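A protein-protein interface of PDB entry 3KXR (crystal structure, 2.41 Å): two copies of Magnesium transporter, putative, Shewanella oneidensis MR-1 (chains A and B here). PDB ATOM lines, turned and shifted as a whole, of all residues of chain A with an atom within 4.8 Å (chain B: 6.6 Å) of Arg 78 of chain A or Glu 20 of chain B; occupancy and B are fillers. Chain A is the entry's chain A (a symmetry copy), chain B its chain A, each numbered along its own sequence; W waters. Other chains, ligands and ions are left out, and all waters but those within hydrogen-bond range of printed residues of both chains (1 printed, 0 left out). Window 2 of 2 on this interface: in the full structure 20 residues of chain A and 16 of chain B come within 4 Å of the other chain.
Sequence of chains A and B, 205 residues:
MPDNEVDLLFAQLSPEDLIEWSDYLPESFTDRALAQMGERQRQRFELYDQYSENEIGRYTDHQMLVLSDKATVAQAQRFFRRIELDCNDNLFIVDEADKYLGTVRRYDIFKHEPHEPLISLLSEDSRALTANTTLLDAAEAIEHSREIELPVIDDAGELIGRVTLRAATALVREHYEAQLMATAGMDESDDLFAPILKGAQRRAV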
ATOM      1  N   ALA A  74       2.822  18.537  15.275  1.00  0.00           N
ATOM      2  CA  ALA A  74       1.808  19.433  14.700  1.00  0.00           C
ATOM      3  C   ALA A  74       0.784  18.643  13.928  1.00  0.00           C
ATOM      4  O   ALA A  74      -0.415  18.868  14.089  1.00  0.00           O
ATOM      5  CB  ALA A  74       2.438  20.499  13.808  1.00  0.00           C
ATOM      6  N   GLN A  75       1.225  17.697  13.112  1.00  0.00           N
ATOM      7  CA  GLN A  75       0.273  16.857  12.370  1.00  0.00           C
ATOM      8  C   GLN A  75      -0.552  15.983  13.289  1.00  0.00           C
ATOM      9  O   GLN A  75      -1.734  15.812  13.072  1.00  0.00           O
ATOM     10  CB  GLN A  75       0.990  15.954  11.368  1.00  0.00           C
ATOM     11  CG  GLN A  75       1.453  16.667  10.102  1.00  0.00           C
ATOM     12  CD  GLN A  75       2.598  17.610  10.376  1.00  0.00           C
ATOM     13  OE1 GLN A  75       3.667  17.192  10.837  1.00  0.00           O
ATOM     14  NE2 GLN A  75       2.365  18.906  10.154  1.00  0.00           N
ATOM     15  N   ALA A  76       0.071  15.418  14.315  1.00  0.00           N
ATOM     16  CA  ALA A  76      -0.622  14.514  15.199  1.00  0.00           C
ATOM     17  C   ALA A  76      -1.689  15.300  15.947  1.00  0.00           C
ATOM     18  O   ALA A  76      -2.826  14.861  16.047  1.00  0.00           O
ATOM     19  CB  ALA A  76       0.326  13.837  16.161  1.00  0.00           C
ATOM     20  N   GLN A  77      -1.345  16.473  16.453  1.00  0.00           N
ATOM     21  CA  GLN A  77      -2.335  17.289  17.183  1.00  0.00           C
ATOM     22  C   GLN A  77      -3.536  17.595  16.310  1.00  0.00           C
ATOM     23  O   GLN A  77      -4.687  17.519  16.759  1.00  0.00           O
ATOM     24  CB  GLN A  77      -1.727  18.606  17.715  1.00  0.00           C
ATOM     25  CG  GLN A  77      -0.867  18.360  18.953  1.00  0.00           C
ATOM     26  CD  GLN A  77      -0.215  19.597  19.504  1.00  0.00           C
ATOM     27  OE1 GLN A  77      -0.479  20.700  19.057  1.00  0.00           O
ATOM     28  NE2 GLN A  77       0.637  19.414  20.499  1.00  0.00           N
ATOM     29  N   ARG A  78      -3.273  17.928  15.065  1.00  0.00           N
ATOM     30  CA  ARG A  78      -4.345  18.291  14.170  1.00  0.00           C
ATOM     31  C   ARG A  78      -5.212  17.061  13.826  1.00  0.00           C
ATOM     32  O   ARG A  78      -6.423  17.165  13.641  1.00  0.00           O
ATOM     33  CB  ARG A  78      -3.741  18.941  12.937  1.00  0.00           C
ATOM     34  CG  ARG A  78      -4.729  19.192  11.867  1.00  0.00           C
ATOM     35  CD  ARG A  78      -4.185  20.104  10.803  1.00  0.00           C
ATOM     36  NE  ARG A  78      -5.233  20.414   9.828  1.00  0.00           N
ATOM     37  CZ  ARG A  78      -4.996  20.750   8.567  1.00  0.00           C
ATOM     38  NH1 ARG A  78      -3.752  20.809   8.115  1.00  0.00           N
ATOM     39  NH2 ARG A  78      -6.000  21.023   7.753  1.00  0.00           N
ATOM     40  N   PHE A  79      -4.602  15.883  13.779  1.00  0.00           N
ATOM     41  CA  PHE A  79      -5.350  14.664  13.473  1.00  0.00           C
ATOM     42  C   PHE A  79      -6.360  14.356  14.579  1.00  0.00           C
ATOM     43  O   PHE A  79      -7.509  13.981  14.331  1.00  0.00           O
ATOM     44  CB  PHE A  79      -4.376  13.477  13.328  1.00  0.00           C
ATOM     45  CG  PHE A  79      -4.711  12.521  12.199  1.00  0.00           C
ATOM     46  CD1 PHE A  79      -6.000  12.391  11.713  1.00  0.00           C
ATOM     47  CD2 PHE A  79      -3.716  11.709  11.666  1.00  0.00           C
ATOM     48  CE1 PHE A  79      -6.283  11.488  10.696  1.00  0.00           C
ATOM     49  CE2 PHE A  79      -3.981  10.793  10.652  1.00  0.00           C
ATOM     50  CZ  PHE A  79      -5.253  10.675  10.159  1.00  0.00           C
ATOM     51  N   PHE A  80      -5.914  14.504  15.814  1.00  0.00           N
ATOM     52  CA  PHE A  80      -6.769  14.199  16.923  1.00  0.00           C
ATOM     53  C   PHE A  80      -7.871  15.227  17.009  1.00  0.00           C
ATOM     54  O   PHE A  80      -8.938  14.909  17.444  1.00  0.00           O
ATOM     55  CB  PHE A  80      -6.006  14.247  18.216  1.00  0.00           C
ATOM     56  CG  PHE A  80      -5.243  13.041  18.511  1.00  0.00           C
ATOM     57  CD1 PHE A  80      -5.888  11.850  18.720  1.00  0.00           C
ATOM     58  CD2 PHE A  80      -3.860  13.099  18.656  1.00  0.00           C
ATOM     59  CE1 PHE A  80      -5.158  10.702  19.014  1.00  0.00           C
ATOM     60  CE2 PHE A  80      -3.130  11.963  18.972  1.00  0.00           C
ATOM     61  CZ  PHE A  80      -3.790  10.758  19.147  1.00  0.00           C
ATOM     62  N   ARG A  81      -7.607  16.464  16.618  1.00  0.00           N
ATOM     63  CA  ARG A  81      -8.623  17.516  16.761  1.00  0.00           C
ATOM     64  C   ARG A  81      -9.635  17.496  15.594  1.00  0.00           C
ATOM     65  O   ARG A  81     -10.782  17.907  15.769  1.00  0.00           O
ATOM     66  CB  ARG A  81      -7.994  18.907  16.932  1.00  0.00           C
ATOM     67  CG  ARG A  81      -7.258  19.146  18.305  1.00  0.00           C
ATOM     68  CD  ARG A  81      -8.180  19.403  19.536  1.00  0.00           C
ATOM     69  N   ARG A  82      -9.240  16.993  14.428  1.00  0.00           N
ATOM     70  CA  ARG A  82     -10.087  17.100  13.238  1.00  0.00           C
ATOM     71  C   ARG A  82     -10.944  15.870  12.955  1.00  0.00           C
ATOM     72  O   ARG A  82     -11.791  15.909  12.118  1.00  0.00           O
ATOM     73  CB  ARG A  82      -9.208  17.349  12.024  1.00  0.00           C
ATOM     74  CG  ARG A  82      -8.511  16.062  11.523  1.00  0.00           C
ATOM     75  CD  ARG A  82      -7.383  16.324  10.532  1.00  0.00           C
ATOM     76  NE  ARG A  82      -7.813  17.094   9.354  1.00  0.00           N
ATOM     77  CZ  ARG A  82      -7.043  17.347   8.289  1.00  0.00           C
ATOM     78  NH1 ARG A  82      -5.787  16.883   8.217  1.00  0.00           N
ATOM     79  NH2 ARG A  82      -7.533  18.076   7.291  1.00  0.00           N
ATOM     80  N   PRO B  15     -10.721  15.157  -0.205  1.00  0.00           N
ATOM     81  CA  PRO B  15      -9.574  14.883  -1.047  1.00  0.00           C
ATOM     82  C   PRO B  15      -8.485  15.958  -0.925  1.00  0.00           C
ATOM     83  O   PRO B  15      -7.299  15.641  -1.086  1.00  0.00           O
ATOM     84  CB  PRO B  15     -10.161  14.818  -2.460  1.00  0.00           C
ATOM     85  CG  PRO B  15     -11.560  15.214  -2.374  1.00  0.00           C
ATOM     86  CD  PRO B  15     -11.964  15.383  -0.965  1.00  0.00           C
ATOM     87  N   GLU B  16      -8.875  17.195  -0.616  1.00  0.00           N
ATOM     88  CA  GLU B  16      -7.908  18.297  -0.410  1.00  0.00           C
ATOM     89  C   GLU B  16      -7.054  18.073   0.831  1.00  0.00           C
ATOM     90  O   GLU B  16      -5.870  18.391   0.850  1.00  0.00           O
ATOM     91  CB  GLU B  16      -8.614  19.663  -0.257  1.00  0.00           C
ATOM     92  CG  GLU B  16      -9.408  20.174  -1.496  1.00  0.00           C
ATOM     93  CD  GLU B  16     -10.884  19.695  -1.565  1.00  0.00           C
ATOM     94  OE1 GLU B  16     -11.300  18.794  -0.811  1.00  0.00           O
ATOM     95  OE2 GLU B  16     -11.634  20.228  -2.408  1.00  0.00           O
ATOM     96  N   ASP B  17      -7.680  17.550   1.879  1.00  0.00           N
ATOM     97  CA  ASP B  17      -6.959  17.194   3.074  1.00  0.00           C
ATOM     98  C   ASP B  17      -5.885  16.185   2.704  1.00  0.00           C
ATOM     99  O   ASP B  17      -4.749  16.302   3.123  1.00  0.00           O
ATOM    100  CB  ASP B  17      -7.911  16.571   4.093  1.00  0.00           C
ATOM    101  CG  ASP B  17      -9.039  17.532   4.543  1.00  0.00           C
ATOM    102  OD1 ASP B  17      -8.904  18.785   4.404  1.00  0.00           O
ATOM    103  OD2 ASP B  17     -10.061  17.008   5.063  1.00  0.00           O
ATOM    104  N   LEU B  18      -6.251  15.194   1.905  1.00  0.00           N
ATOM    105  CA  LEU B  18      -5.308  14.149   1.545  1.00  0.00           C
ATOM    106  C   LEU B  18      -4.105  14.741   0.841  1.00  0.00           C
ATOM    107  O   LEU B  18      -2.981  14.421   1.190  1.00  0.00           O
ATOM    108  CB  LEU B  18      -5.965  13.068   0.686  1.00  0.00           C
ATOM    109  CG  LEU B  18      -7.032  12.195   1.364  1.00  0.00           C
ATOM    110  CD1 LEU B  18      -7.682  11.244   0.347  1.00  0.00           C
ATOM    111  CD2 LEU B  18      -6.449  11.387   2.555  1.00  0.00           C
ATOM    112  N   ILE B  19      -4.352  15.652  -0.095  1.00  0.00           N
ATOM    113  CA  ILE B  19      -3.298  16.307  -0.873  1.00  0.00           C
ATOM    114  C   ILE B  19      -2.380  17.120   0.020  1.00  0.00           C
ATOM    115  O   ILE B  19      -1.134  17.012  -0.042  1.00  0.00           O
ATOM    116  CB  ILE B  19      -3.877  17.226  -1.979  1.00  0.00           C
ATOM    117  CG1 ILE B  19      -4.524  16.387  -3.086  1.00  0.00           C
ATOM    118  CG2 ILE B  19      -2.787  18.121  -2.579  1.00  0.00           C
ATOM    119  CD1 ILE B  19      -3.523  15.713  -4.024  1.00  0.00           C
ATOM    120  N   GLU B  20      -3.007  17.901   0.884  1.00  0.00           N
ATOM    121  CA  GLU B  20      -2.260  18.743   1.782  1.00  0.00           C
ATOM    122  C   GLU B  20      -1.387  17.891   2.709  1.00  0.00           C
ATOM    123  O   GLU B  20      -0.291  18.300   3.087  1.00  0.00           O
ATOM    124  CB  GLU B  20      -3.233  19.573   2.584  1.00  0.00           C
ATOM    125  CG  GLU B  20      -2.583  20.495   3.594  1.00  0.00           C
ATOM    126  CD  GLU B  20      -3.538  20.858   4.694  1.00  0.00           C
ATOM    127  OE1 GLU B  20      -4.742  20.541   4.549  1.00  0.00           O
ATOM    128  OE2 GLU B  20      -3.083  21.450   5.706  1.00  0.00           O
ATOM    129  N   TRP B  21      -1.858  16.697   3.044  1.00  0.00           N
ATOM    130  CA  TRP B  21      -1.120  15.797   3.925  1.00  0.00           C
ATOM    131  C   TRP B  21      -0.392  14.653   3.232  1.00  0.00           C
ATOM    132  O   TRP B  21      -0.115  13.606   3.847  1.00  0.00           O
ATOM    133  CB  TRP B  21      -2.079  15.265   4.969  1.00  0.00           C
ATOM    134  CG  TRP B  21      -2.011  16.057   6.182  1.00  0.00           C
ATOM    135  CD1 TRP B  21      -1.452  17.294   6.330  1.00  0.00           C
ATOM    136  CD2 TRP B  21      -2.503  15.684   7.449  1.00  0.00           C
ATOM    137  NE1 TRP B  21      -1.556  17.703   7.617  1.00  0.00           N
ATOM    138  CE2 TRP B  21      -2.197  16.728   8.335  1.00  0.00           C
ATOM    139  CE3 TRP B  21      -3.160  14.555   7.934  1.00  0.00           C
ATOM    140  CZ2 TRP B  21      -2.535  16.686   9.686  1.00  0.00           C
ATOM    141  CZ3 TRP B  21      -3.499  14.505   9.288  1.00  0.00           C
ATOM    142  CH2 TRP B  21      -3.192  15.563  10.145  1.00  0.00           C
ATOM    143  N   SER B  22      -0.053  14.873   1.964  1.00  0.00           N
ATOM    144  CA  SER B  22       0.567  13.828   1.156  1.00  0.00           C
ATOM    145  C   SER B  22       1.962  13.465   1.637  1.00  0.00           C
ATOM    146  O   SER B  22       2.347  12.327   1.504  1.00  0.00           O
ATOM    147  CB  SER B  22       0.546  14.161  -0.346  1.00  0.00           C
ATOM    148  OG  SER B  22       1.334  15.281  -0.654  1.00  0.00           O
ATOM    149  N   ASP B  23       2.694  14.389   2.258  1.00  0.00           N
ATOM    150  CA  ASP B  23       3.990  14.019   2.885  1.00  0.00           C
ATOM    151  C   ASP B  23       3.876  13.205   4.148  1.00  0.00           C
ATOM    152  O   ASP B  23       4.879  12.723   4.618  1.00  0.00           O
ATOM    153  CB  ASP B  23       4.854  15.265   3.218  1.00  0.00           C
ATOM    154  CG  ASP B  23       5.220  16.093   1.962  1.00  0.00           C
ATOM    155  OD1 ASP B  23       5.244  15.543   0.835  1.00  0.00           O
ATOM    156  OD2 ASP B  23       5.459  17.303   2.089  1.00  0.00           O
ATOM    157  N   TYR B  24       2.688  13.076   4.736  1.00  0.00           N
ATOM    158  CA  TYR B  24       2.595  12.534   6.089  1.00  0.00           C
ATOM    159  C   TYR B  24       1.743  11.285   6.207  1.00  0.00           C
ATOM    160  O   TYR B  24       1.864  10.559   7.168  1.00  0.00           O
ATOM    161  CB  TYR B  24       2.055  13.595   7.059  1.00  0.00           C
ATOM    162  CG  TYR B  24       2.732  14.932   6.951  1.00  0.00           C
ATOM    163  CD1 TYR B  24       4.050  15.072   7.291  1.00  0.00           C
ATOM    164  CD2 TYR B  24       2.039  16.064   6.502  1.00  0.00           C
ATOM    165  CE1 TYR B  24       4.687  16.294   7.185  1.00  0.00           C
ATOM    166  CE2 TYR B  24       2.670  17.293   6.402  1.00  0.00           C
ATOM    167  CZ  TYR B  24       3.992  17.396   6.735  1.00  0.00           C
ATOM    168  OH  TYR B  24       4.652  18.603   6.635  1.00  0.00           O
HETATM  169  O   HOH W   1      -4.777  18.109   5.716  1.00  0.00           O
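Among the printed residues, pairs that only touch across the chains: Gln 75 of chain A with Trp 21 of chain B (3.3 Å), Arg 82 of chain A with Trp 21 of chain B (3.5 Å), Phe 79 of chain A with Trp 21 of chain B (3.7 Å), Gln 75 of chain A with Tyr 24 of chain B (3.7 Å) and Arg 78 of chain A with Trp 21 of chain B (3.8 Å).
Of the printed residues of chain B, Gln 75 of chain A touches Trp 21 (3.3 Å) and Tyr 24 (3.7 Å). Of the printed residues of chain B, Arg 82 of chain A touches Asp 17 and Trp 21. Of the printed residues of chain A, Asp 17 of chain B touches Arg 82 (3.2 Å). Of the printed residues of chain A, Trp 21 of chain B touches Gln 75 (3.3 Å), Arg 78 (3.8 Å), Phe 79 (3.7 Å) and Arg 82 (3.5 Å). Printed residues of chain A within 4 Å of Tyr 24 of chain B: Gln 75. The nearest residue of chain A that does not touch Glu 20 of chain B is Arg 82 of chain A (4.6 Å). The nearest printed residue of chain B that does not touch Gln 75 of chain A is Asp 23 of chain B (7.3 Å).
Water W1 lies within hydrogen-bond range of OE1 of Glu 20 of chain B (2.7 Å), NH1 of Arg 82 of chain A (3.0 Å) and O of Asp 17 of chain B (3.2 Å).
No position is printed for both chains. Of the 7 pairs that touch across the chains among the printed residues, none has its exchanged pair printed and touching as well.
The side-chain carboxylate (OD1) of Asp 17 of chain B lies within salt-bridge range of the guanidinium group (NH2) of Arg 82 of chain A (3.3 Å). NH1 of Arg 78 of chain A is in salt-bridge range of OE2 of Glu 20 of chain B (2.6 Å).
Of the 10 printed residues of chain B, 4 touch a printed residue of chain A.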
